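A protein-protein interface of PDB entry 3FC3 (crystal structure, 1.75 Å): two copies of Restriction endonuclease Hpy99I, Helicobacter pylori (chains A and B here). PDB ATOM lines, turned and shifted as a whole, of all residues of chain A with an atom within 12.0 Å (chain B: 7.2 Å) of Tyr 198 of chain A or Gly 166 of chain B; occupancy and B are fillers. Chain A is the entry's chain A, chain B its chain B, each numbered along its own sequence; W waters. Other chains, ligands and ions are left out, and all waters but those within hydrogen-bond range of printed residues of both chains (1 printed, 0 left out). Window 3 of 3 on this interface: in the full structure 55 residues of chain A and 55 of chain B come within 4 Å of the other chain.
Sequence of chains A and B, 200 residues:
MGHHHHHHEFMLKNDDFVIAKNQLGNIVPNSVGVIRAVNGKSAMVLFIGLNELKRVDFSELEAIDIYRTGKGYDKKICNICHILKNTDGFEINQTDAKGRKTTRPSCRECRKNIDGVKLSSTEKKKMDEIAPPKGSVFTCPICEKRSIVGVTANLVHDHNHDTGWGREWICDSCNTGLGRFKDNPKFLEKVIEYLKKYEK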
ATOM      1  N   GLU A 189     -25.013   3.069  -6.019  1.00  0.00           N
ATOM      2  CA  GLU A 189     -23.774   3.197  -5.265  1.00  0.00           C
ATOM      3  C   GLU A 189     -22.756   2.161  -5.732  1.00  0.00           C
ATOM      4  O   GLU A 189     -21.570   2.458  -5.845  1.00  0.00           O
ATOM      5  CB  GLU A 189     -24.034   3.066  -3.766  1.00  0.00           C
ATOM      6  CG  GLU A 189     -24.812   4.228  -3.165  1.00  0.00           C
ATOM      7  CD  GLU A 189     -23.970   5.472  -2.983  1.00  0.00           C
ATOM      8  OE1 GLU A 189     -22.838   5.508  -3.527  1.00  0.00           O
ATOM      9  OE2 GLU A 189     -24.435   6.416  -2.291  1.00  0.00           O
ATOM     10  N   LYS A 190     -23.231   0.953  -6.034  1.00  0.00           N
ATOM     11  CA  LYS A 190     -22.375  -0.088  -6.594  1.00  0.00           C
ATOM     12  C   LYS A 190     -21.807   0.323  -7.946  1.00  0.00           C
ATOM     13  O   LYS A 190     -20.625   0.086  -8.235  1.00  0.00           O
ATOM     14  CB  LYS A 190     -23.146  -1.408  -6.701  1.00  0.00           C
ATOM     15  CG  LYS A 190     -23.371  -2.037  -5.340  1.00  0.00           C
ATOM     16  CD  LYS A 190     -23.674  -3.477  -5.442  1.00  0.00           C
ATOM     17  CE  LYS A 190     -22.433  -4.290  -5.787  1.00  0.00           C
ATOM     18  NZ  LYS A 190     -22.841  -5.559  -6.390  1.00  0.00           N
ATOM     19  N   VAL A 191     -22.643   0.948  -8.770  1.00  0.00           N
ATOM     20  CA  VAL A 191     -22.175   1.462 -10.051  1.00  0.00           C
ATOM     21  C   VAL A 191     -21.044   2.489  -9.871  1.00  0.00           C
ATOM     22  O   VAL A 191     -20.031   2.448 -10.578  1.00  0.00           O
ATOM     23  CB  VAL A 191     -23.313   2.128 -10.855  1.00  0.00           C
ATOM     24  CG1 VAL A 191     -22.754   2.754 -12.117  1.00  0.00           C
ATOM     25  CG2 VAL A 191     -24.407   1.104 -11.182  1.00  0.00           C
ATOM     26  N   ILE A 192     -21.238   3.413  -8.930  1.00  0.00           N
ATOM     27  CA  ILE A 192     -20.256   4.478  -8.669  1.00  0.00           C
ATOM     28  C   ILE A 192     -18.908   3.878  -8.289  1.00  0.00           C
ATOM     29  O   ILE A 192     -17.877   4.256  -8.842  1.00  0.00           O
ATOM     30  CB  ILE A 192     -20.750   5.471  -7.570  1.00  0.00           C
ATOM     31  CG1 ILE A 192     -21.881   6.343  -8.128  1.00  0.00           C
ATOM     32  CG2 ILE A 192     -19.603   6.358  -7.062  1.00  0.00           C
ATOM     33  CD1 ILE A 192     -22.649   7.093  -7.077  1.00  0.00           C
ATOM     34  N   GLU A 193     -18.925   2.915  -7.373  1.00  0.00           N
ATOM     35  CA  GLU A 193     -17.678   2.317  -6.894  1.00  0.00           C
ATOM     36  C   GLU A 193     -17.020   1.458  -7.972  1.00  0.00           C
ATOM     37  O   GLU A 193     -15.797   1.405  -8.065  1.00  0.00           O
ATOM     38  CB  GLU A 193     -17.924   1.528  -5.601  1.00  0.00           C
ATOM     39  CG  GLU A 193     -18.436   2.412  -4.446  1.00  0.00           C
ATOM     40  CD  GLU A 193     -17.559   3.663  -4.180  1.00  0.00           C
ATOM     41  OE1 GLU A 193     -16.312   3.525  -4.039  1.00  0.00           O
ATOM     42  OE2 GLU A 193     -18.113   4.792  -4.097  1.00  0.00           O
ATOM     43  N   TYR A 194     -17.841   0.815  -8.801  1.00  0.00           N
ATOM     44  CA  TYR A 194     -17.362   0.074  -9.966  1.00  0.00           C
ATOM     45  C   TYR A 194     -16.657   0.986 -10.966  1.00  0.00           C
ATOM     46  O   TYR A 194     -15.580   0.651 -11.465  1.00  0.00           O
ATOM     47  CB  TYR A 194     -18.547  -0.617 -10.647  1.00  0.00           C
ATOM     48  CG  TYR A 194     -18.249  -1.347 -11.940  1.00  0.00           C
ATOM     49  CD1 TYR A 194     -17.761  -2.638 -11.938  1.00  0.00           C
ATOM     50  CD2 TYR A 194     -18.506  -0.756 -13.173  1.00  0.00           C
ATOM     51  CE1 TYR A 194     -17.519  -3.322 -13.146  1.00  0.00           C
ATOM     52  CE2 TYR A 194     -18.270  -1.429 -14.378  1.00  0.00           C
ATOM     53  CZ  TYR A 194     -17.774  -2.704 -14.365  1.00  0.00           C
ATOM     54  OH  TYR A 194     -17.529  -3.373 -15.545  1.00  0.00           O
ATOM     55  N   LEU A 195     -17.280   2.120 -11.281  1.00  0.00           N
ATOM     56  CA  LEU A 195     -16.710   3.053 -12.269  1.00  0.00           C
ATOM     57  C   LEU A 195     -15.436   3.679 -11.721  1.00  0.00           C
ATOM     58  O   LEU A 195     -14.415   3.726 -12.415  1.00  0.00           O
ATOM     59  CB  LEU A 195     -17.720   4.149 -12.643  1.00  0.00           C
ATOM     60  CG  LEU A 195     -18.943   3.690 -13.428  1.00  0.00           C
ATOM     61  CD1 LEU A 195     -19.961   4.818 -13.577  1.00  0.00           C
ATOM     62  CD2 LEU A 195     -18.531   3.151 -14.786  1.00  0.00           C
ATOM     63  N   LYS A 196     -15.518   4.132 -10.468  1.00  0.00           N
ATOM     64  CA  LYS A 196     -14.398   4.767  -9.763  1.00  0.00           C
ATOM     65  C   LYS A 196     -13.184   3.850  -9.724  1.00  0.00           C
ATOM     66  O   LYS A 196     -12.065   4.288  -9.957  1.00  0.00           O
ATOM     67  CB  LYS A 196     -14.817   5.171  -8.344  1.00  0.00           C
ATOM     68  CG  LYS A 196     -15.672   6.452  -8.290  1.00  0.00           C
ATOM     69  CD  LYS A 196     -15.757   7.017  -6.875  1.00  0.00           C
ATOM     70  CE  LYS A 196     -14.534   7.867  -6.545  1.00  0.00           C
ATOM     71  NZ  LYS A 196     -14.166   7.879  -5.082  1.00  0.00           N
ATOM     72  N   LYS A 197     -13.429   2.569  -9.467  1.00  0.00           N
ATOM     73  CA  LYS A 197     -12.398   1.542  -9.467  1.00  0.00           C
ATOM     74  C   LYS A 197     -11.572   1.479 -10.774  1.00  0.00           C
ATOM     75  O   LYS A 197     -10.384   1.154 -10.739  1.00  0.00           O
ATOM     76  CB  LYS A 197     -13.058   0.183  -9.171  1.00  0.00           C
ATOM     77  CG  LYS A 197     -12.148  -1.020  -9.274  1.00  0.00           C
ATOM     78  CD  LYS A 197     -12.777  -2.254  -8.651  1.00  0.00           C
ATOM     79  CE  LYS A 197     -11.856  -3.458  -8.797  1.00  0.00           C
ATOM     80  NZ  LYS A 197     -12.342  -4.636  -8.019  1.00  0.00           N
ATOM     81  N   TYR A 198     -12.189   1.798 -11.915  1.00  0.00           N
ATOM     82  CA  TYR A 198     -11.520   1.696 -13.226  1.00  0.00           C
ATOM     83  C   TYR A 198     -11.244   3.047 -13.901  1.00  0.00           C
ATOM     84  O   TYR A 198     -10.904   3.081 -15.090  1.00  0.00           O
ATOM     85  CB  TYR A 198     -12.355   0.804 -14.165  1.00  0.00           C
ATOM     86  CG  TYR A 198     -12.379  -0.639 -13.717  1.00  0.00           C
ATOM     87  CD1 TYR A 198     -11.255  -1.436 -13.861  1.00  0.00           C
ATOM     88  CD2 TYR A 198     -13.512  -1.197 -13.128  1.00  0.00           C
ATOM     89  CE1 TYR A 198     -11.247  -2.754 -13.434  1.00  0.00           C
ATOM     90  CE2 TYR A 198     -13.520  -2.512 -12.698  1.00  0.00           C
ATOM     91  CZ  TYR A 198     -12.380  -3.290 -12.850  1.00  0.00           C
ATOM     92  OH  TYR A 198     -12.360  -4.608 -12.429  1.00  0.00           O
ATOM     93  N   GLU A 199     -11.383   4.141 -13.146  1.00  0.00           N
ATOM     94  CA  GLU A 199     -11.185   5.502 -13.686  1.00  0.00           C
ATOM     95  C   GLU A 199      -9.723   5.810 -14.030  1.00  0.00           C
ATOM     96  O   GLU A 199      -8.806   5.126 -13.571  1.00  0.00           O
ATOM     97  CB  GLU A 199     -11.706   6.559 -12.700  1.00  0.00           C
ATOM     98  CG  GLU A 199     -13.124   7.034 -12.981  1.00  0.00           C
ATOM     99  CD  GLU A 199     -13.601   8.091 -11.983  1.00  0.00           C
ATOM    100  OE1 GLU A 199     -12.993   8.216 -10.879  1.00  0.00           O
ATOM    101  OE2 GLU A 199     -14.590   8.794 -12.308  1.00  0.00           O
ATOM    102  N   LEU B 119     -12.280  -0.644 -26.792  1.00  0.00           N
ATOM    103  CA  LEU B 119     -11.533  -1.629 -26.019  1.00  0.00           C
ATOM    104  C   LEU B 119     -10.379  -2.116 -26.876  1.00  0.00           C
ATOM    105  O   LEU B 119     -10.573  -2.525 -28.021  1.00  0.00           O
ATOM    106  CB  LEU B 119     -12.431  -2.817 -25.634  1.00  0.00           C
ATOM    107  CG  LEU B 119     -11.769  -3.937 -24.825  1.00  0.00           C
ATOM    108  CD1 LEU B 119     -11.379  -3.454 -23.444  1.00  0.00           C
ATOM    109  CD2 LEU B 119     -12.687  -5.156 -24.737  1.00  0.00           C
ATOM    110  N   SER B 120      -9.173  -2.053 -26.324  1.00  0.00           N
ATOM    111  CA  SER B 120      -7.979  -2.461 -27.052  1.00  0.00           C
ATOM    112  C   SER B 120      -7.918  -3.981 -27.191  1.00  0.00           C
ATOM    113  O   SER B 120      -8.498  -4.711 -26.384  1.00  0.00           O
ATOM    114  CB  SER B 120      -6.727  -1.956 -26.340  1.00  0.00           C
ATOM    115  OG  SER B 120      -6.411  -2.755 -25.213  1.00  0.00           O
ATOM    116  N   GLU B 123      -6.359  -5.660 -24.085  1.00  0.00           N
ATOM    117  CA  GLU B 123      -7.348  -5.635 -23.005  1.00  0.00           C
ATOM    118  C   GLU B 123      -8.496  -6.617 -23.284  1.00  0.00           C
ATOM    119  O   GLU B 123      -8.966  -7.267 -22.363  1.00  0.00           O
ATOM    120  CB  GLU B 123      -7.874  -4.214 -22.760  1.00  0.00           C
ATOM    121  CG  GLU B 123      -6.865  -3.291 -22.096  1.00  0.00           C
ATOM    122  CD  GLU B 123      -6.593  -3.655 -20.645  1.00  0.00           C
ATOM    123  OE1 GLU B 123      -5.419  -3.955 -20.330  1.00  0.00           O
ATOM    124  OE2 GLU B 123      -7.534  -3.675 -19.815  1.00  0.00           O
ATOM    125  N   LYS B 124      -8.911  -6.742 -24.547  1.00  0.00           N
ATOM    126  CA  LYS B 124      -9.955  -7.702 -24.928  1.00  0.00           C
ATOM    127  C   LYS B 124      -9.506  -9.152 -24.680  1.00  0.00           C
ATOM    128  O   LYS B 124     -10.278  -9.992 -24.194  1.00  0.00           O
ATOM    129  CB  LYS B 124     -10.387  -7.531 -26.387  1.00  0.00           C
ATOM    130  CG  LYS B 124     -11.611  -8.396 -26.744  1.00  0.00           C
ATOM    131  CD  LYS B 124     -12.171  -8.140 -28.131  1.00  0.00           C
ATOM    132  CE  LYS B 124     -13.559  -8.802 -28.291  1.00  0.00           C
ATOM    133  NZ  LYS B 124     -14.191  -8.521 -29.622  1.00  0.00           N
ATOM    134  N   MET B 127      -9.601 -10.001 -21.025  1.00  0.00           N
ATOM    135  CA  MET B 127     -10.972 -10.281 -20.591  1.00  0.00           C
ATOM    136  C   MET B 127     -11.432 -11.662 -21.073  1.00  0.00           C
ATOM    137  O   MET B 127     -12.086 -12.404 -20.337  1.00  0.00           O
ATOM    138  CB  MET B 127     -11.912  -9.177 -21.083  1.00  0.00           C
ATOM    139  CG  MET B 127     -11.638  -7.839 -20.417  1.00  0.00           C
ATOM    140  SD  MET B 127     -12.916  -6.612 -20.733  1.00  0.00           S
ATOM    141  CE  MET B 127     -14.196  -7.189 -19.615  1.00  0.00           C
ATOM    142  N   HIS B 157     -18.345  -7.581 -22.589  1.00  0.00           N
ATOM    143  CA  HIS B 157     -17.055  -6.992 -22.218  1.00  0.00           C
ATOM    144  C   HIS B 157     -17.278  -5.511 -21.975  1.00  0.00           C
ATOM    145  O   HIS B 157     -17.353  -4.776 -22.949  1.00  0.00           O
ATOM    146  CB  HIS B 157     -16.044  -7.046 -23.388  1.00  0.00           C
ATOM    147  CG  HIS B 157     -15.617  -8.406 -23.810  1.00  0.00           C
ATOM    148  ND1 HIS B 157     -16.289  -9.126 -24.774  1.00  0.00           N
ATOM    149  CD2 HIS B 157     -14.518  -9.129 -23.497  1.00  0.00           C
ATOM    150  CE1 HIS B 157     -15.658 -10.268 -24.987  1.00  0.00           C
ATOM    151  NE2 HIS B 157     -14.580 -10.294 -24.223  1.00  0.00           N
ATOM    152  N   ASP B 158     -17.402  -5.063 -20.729  1.00  0.00           N
ATOM    153  CA  ASP B 158     -17.481  -3.616 -20.445  1.00  0.00           C
ATOM    154  C   ASP B 158     -16.070  -3.026 -20.462  1.00  0.00           C
ATOM    155  O   ASP B 158     -15.120  -3.703 -20.086  1.00  0.00           O
ATOM    156  CB  ASP B 158     -18.152  -3.407 -19.096  1.00  0.00           C
ATOM    157  CG  ASP B 158     -18.233  -1.967 -18.685  1.00  0.00           C
ATOM    158  OD1 ASP B 158     -18.490  -1.080 -19.521  1.00  0.00           O
ATOM    159  OD2 ASP B 158     -18.084  -1.715 -17.485  1.00  0.00           O
ATOM    160  N   HIS B 159     -15.936  -1.774 -20.918  1.00  0.00           N
ATOM    161  CA  HIS B 159     -14.634  -1.117 -20.935  1.00  0.00           C
ATOM    162  C   HIS B 159     -14.778   0.358 -20.665  1.00  0.00           C
ATOM    163  O   HIS B 159     -15.853   0.936 -20.859  1.00  0.00           O
ATOM    164  CB  HIS B 159     -13.934  -1.336 -22.280  1.00  0.00           C
ATOM    165  CG  HIS B 159     -14.390  -0.421 -23.368  1.00  0.00           C
ATOM    166  ND1 HIS B 159     -15.597  -0.574 -24.017  1.00  0.00           N
ATOM    167  CD2 HIS B 159     -13.793   0.664 -23.928  1.00  0.00           C
ATOM    168  CE1 HIS B 159     -15.722   0.372 -24.935  1.00  0.00           C
ATOM    169  NE2 HIS B 159     -14.643   1.137 -24.900  1.00  0.00           N
ATOM    170  N   ASN B 160     -13.683   0.955 -20.212  1.00  0.00           N
ATOM    171  CA  ASN B 160     -13.631   2.389 -19.988  1.00  0.00           C
ATOM    172  C   ASN B 160     -13.349   3.091 -21.335  1.00  0.00           C
ATOM    173  O   ASN B 160     -12.357   2.787 -22.000  1.00  0.00           O
ATOM    174  CB  ASN B 160     -12.569   2.701 -18.920  1.00  0.00           C
ATOM    175  CG  ASN B 160     -12.492   4.166 -18.593  1.00  0.00           C
ATOM    176  OD1 ASN B 160     -12.154   4.972 -19.451  1.00  0.00           O
ATOM    177  ND2 ASN B 160     -12.838   4.528 -17.354  1.00  0.00           N
ATOM    178  N   THR B 163     -10.039   5.541 -21.589  1.00  0.00           N
ATOM    179  CA  THR B 163      -8.719   4.882 -21.646  1.00  0.00           C
ATOM    180  C   THR B 163      -8.642   3.720 -22.648  1.00  0.00           C
ATOM    181  O   THR B 163      -7.570   3.426 -23.179  1.00  0.00           O
ATOM    182  CB  THR B 163      -8.330   4.331 -20.270  1.00  0.00           C
ATOM    183  OG1 THR B 163      -9.263   3.310 -19.880  1.00  0.00           O
ATOM    184  CG2 THR B 163      -8.308   5.443 -19.229  1.00  0.00           C
ATOM    185  N   GLY B 164      -9.765   3.048 -22.895  1.00  0.00           N
ATOM    186  CA  GLY B 164      -9.777   1.875 -23.756  1.00  0.00           C
ATOM    187  C   GLY B 164      -9.445   0.598 -23.000  1.00  0.00           C
ATOM    188  O   GLY B 164      -9.266  -0.453 -23.602  1.00  0.00           O
ATOM    189  N   TRP B 165      -9.365   0.695 -21.675  1.00  0.00           N
ATOM    190  CA  TRP B 165      -9.049  -0.443 -20.825  1.00  0.00           C
ATOM    191  C   TRP B 165     -10.315  -1.183 -20.414  1.00  0.00           C
ATOM    192  O   TRP B 165     -11.377  -0.593 -20.315  1.00  0.00           O
ATOM    193  CB  TRP B 165      -8.285   0.022 -19.593  1.00  0.00           C
ATOM    194  CG  TRP B 165      -6.962   0.665 -19.967  1.00  0.00           C
ATOM    195  CD1 TRP B 165      -6.238   0.446 -21.117  1.00  0.00           C
ATOM    196  CD2 TRP B 165      -6.207   1.615 -19.198  1.00  0.00           C
ATOM    197  NE1 TRP B 165      -5.100   1.208 -21.113  1.00  0.00           N
ATOM    198  CE2 TRP B 165      -5.051   1.936 -19.951  1.00  0.00           C
ATOM    199  CE3 TRP B 165      -6.399   2.236 -17.958  1.00  0.00           C
ATOM    200  CZ2 TRP B 165      -4.082   2.847 -19.495  1.00  0.00           C
ATOM    201  CZ3 TRP B 165      -5.442   3.141 -17.507  1.00  0.00           C
ATOM    202  CH2 TRP B 165      -4.296   3.437 -18.276  1.00  0.00           C
ATOM    203  N   GLY B 166     -10.176  -2.477 -20.162  1.00  0.00           N
ATOM    204  CA  GLY B 166     -11.303  -3.299 -19.790  1.00  0.00           C
ATOM    205  C   GLY B 166     -11.733  -2.990 -18.380  1.00  0.00           C
ATOM    206  O   GLY B 166     -10.929  -2.536 -17.560  1.00  0.00           O
ATOM    207  N   ARG B 167     -13.018  -3.206 -18.105  1.00  0.00           N
ATOM    208  CA  ARG B 167     -13.505  -3.223 -16.748  1.00  0.00           C
ATOM    209  C   ARG B 167     -13.812  -4.693 -16.386  1.00  0.00           C
ATOM    210  O   ARG B 167     -12.882  -5.483 -16.237  1.00  0.00           O
ATOM    211  CB  ARG B 167     -14.674  -2.254 -16.588  1.00  0.00           C
ATOM    212  CG  ARG B 167     -14.227  -0.800 -16.827  1.00  0.00           C
ATOM    213  CD  ARG B 167     -15.162   0.207 -16.205  1.00  0.00           C
ATOM    214  NE  ARG B 167     -16.351   0.406 -17.038  1.00  0.00           N
ATOM    215  CZ  ARG B 167     -16.746   1.562 -17.561  1.00  0.00           C
ATOM    216  NH1 ARG B 167     -16.068   2.697 -17.362  1.00  0.00           N
ATOM    217  NH2 ARG B 167     -17.844   1.588 -18.280  1.00  0.00           N
ATOM    218  N   GLU B 168     -15.078  -5.070 -16.265  1.00  0.00           N
ATOM    219  CA  GLU B 168     -15.434  -6.430 -15.889  1.00  0.00           C
ATOM    220  C   GLU B 168     -16.506  -6.980 -16.818  1.00  0.00           C
ATOM    221  O   GLU B 168     -17.144  -6.252 -17.566  1.00  0.00           O
ATOM    222  CB  GLU B 168     -15.925  -6.495 -14.442  1.00  0.00           C
ATOM    223  CG  GLU B 168     -14.875  -6.047 -13.451  1.00  0.00           C
ATOM    224  CD  GLU B 168     -15.349  -5.982 -12.013  1.00  0.00           C
ATOM    225  OE1 GLU B 168     -16.403  -6.553 -11.675  1.00  0.00           O
ATOM    226  OE2 GLU B 168     -14.641  -5.342 -11.208  1.00  0.00           O
ATOM    227  N   TRP B 169     -16.666  -8.292 -16.767  1.00  0.00           N
ATOM    228  CA  TRP B 169     -17.810  -8.948 -17.387  1.00  0.00           C
ATOM    229  C   TRP B 169     -19.042  -8.615 -16.571  1.00  0.00           C
ATOM    230  O   TRP B 169     -19.078  -8.868 -15.360  1.00  0.00           O
ATOM    231  CB  TRP B 169     -17.599 -10.453 -17.429  1.00  0.00           C
ATOM    232  CG  TRP B 169     -16.639 -10.877 -18.489  1.00  0.00           C
ATOM    233  CD1 TRP B 169     -15.280 -11.082 -18.360  1.00  0.00           C
ATOM    234  CD2 TRP B 169     -16.967 -11.168 -19.834  1.00  0.00           C
ATOM    235  NE1 TRP B 169     -14.755 -11.479 -19.573  1.00  0.00           N
ATOM    236  CE2 TRP B 169     -15.773 -11.542 -20.490  1.00  0.00           C
ATOM    237  CE3 TRP B 169     -18.163 -11.136 -20.565  1.00  0.00           C
ATOM    238  CZ2 TRP B 169     -15.744 -11.875 -21.843  1.00  0.00           C
ATOM    239  CZ3 TRP B 169     -18.133 -11.470 -21.913  1.00  0.00           C
ATOM    240  CH2 TRP B 169     -16.936 -11.853 -22.534  1.00  0.00           C
HETATM  241  O   HOH W   1     -14.635   3.890 -15.083  1.00  0.00           O
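Tyr 198 of chain A touches just these residues of chain B: Asn 160 (3.3 Å), Gly 166 (3.9 Å), Arg 167 (3.5 Å) and Glu 168 (2.7 Å).
Printed residues of chain A within 4 Å of Gly 166 of chain B: Tyr 198 (3.9 Å).
No residue of chain A comes within 4 Å of Glu 123 of chain B.
Of chain A, only Tyr 194 comes within 4 Å of Asp 158 of chain B.
His 159 of chain B touches none of the printed residues of chain A.
Asn 160 of chain B touches one residue of chain A.
No residue of chain A comes within 4 Å of Gly 164 of chain B.
Of chain A, only Tyr 194 (3.2 Å), Leu 195 (3.6 Å) and Tyr 198 (3.5 Å) come within 4 Å of Arg 167 of chain B.
Printed residues of chain B within 4 Å of Lys 197 of chain A: Glu 168.
Of the printed residues of chain B, Tyr 194 of chain A touches Asp 158, Arg 167 and Glu 168.
Glu 189 of chain A touches none of the printed residues of chain B.
The nearest residue of chain A that does not touch Gly 166 of chain B is Tyr 194 of chain A (6.5 Å).
The nearest printed residue of chain B that does not touch Tyr 194 of chain A is Trp 169 of chain B (5.1 Å).
Of the 11 printed residues of chain A, 4 touch a printed residue of chain B.
Hydrophobic or aromatic side chains of chain A that line the printed part of chain B: Tyr 194, Leu 195 and Tyr 198.
Of the 16 printed residues of chain B, 5 touch a printed residue of chain A.
Among the printed residues, Asp or Glu carboxylates within 4 Å of a Lys or Arg side-chain nitrogen of the other chain: Lys 197 of chain A with Glu 168 of chain B.
Water W1 lies within hydrogen-bond range of the backbone carbonyl oxygen of Leu 195 of chain A (2.7 Å), the guanidinium group of Arg 167 of chain B (2.9 Å) and the side-chain amide nitrogen of Asn 160 of chain B (3.0 Å).
Tyr 194 of chain A touches Arg 167 of chain B.
Arg 167 of chain B touches Leu 195 of chain A.
Gly 166 of chain B touches Tyr 198 of chain A.
CD of Arg 167 of chain B touches CB of Tyr 198 of chain A (3.5 Å).
The side-chain carboxylate (OE2) of Glu 123 of chain B lies within hydrogen-bond range of the backbone NH (N) of Gly 166 of chain B, 2.9 Å away.
The guanidinium group (NE) of Arg 167 of chain B lies within salt-bridge range of the side-chain carboxylate (OD2) of Asp 158 of chain B, 2.8 Å away.
The backbone NH of Asp 158 of chain B sits close to the backbone carbonyl oxygen of Glu 168 of chain B, at 3.4 Å.
The backbone carbonyl oxygen of His 159 of chain B is in hydrogen-bond range of the guanidinium group of Arg 167 of chain B (3.3 Å).
The backbone NH (N) of Thr 163 of chain B sits at hydrogen-bond distance from the side-chain amide oxygen (OD1) of Asn 160 of chain B (3.1 Å).
The backbone carbonyl oxygen (O) of Trp 165 of chain B sits at hydrogen-bond distance from the backbone NH (N) of Asn 160 of chain B (2.8 Å).
No position is printed for both chains.
Of the 9 pairs that touch across the chains among the printed residues, none has its exchanged pair printed and touching as well.
OH of Tyr 194 of chain A is in hydrogen-bond range of OD2 of Asp 158 of chain B, at 2.6 Å.
The side-chain hydroxyl (OH) of Tyr 194 of chain A is in hydrogen-bond range of the backbone NH (N) of Glu 168 of chain B.
The side-chain amino group of Lys 197 of chain A is in salt-bridge range of the side-chain carboxylate of Glu 168 of chain B (3.99 Å).
O of Tyr 198 of chain A lies within hydrogen-bond range of ND2 of Asn 160 of chain B, at 3.3 Å.
The side-chain carboxylate (OE2) of Glu 168 of chain B lies within hydrogen-bond range of the side-chain hydroxyl (OH) of Tyr 198 of chain A, at 2.7 Å.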
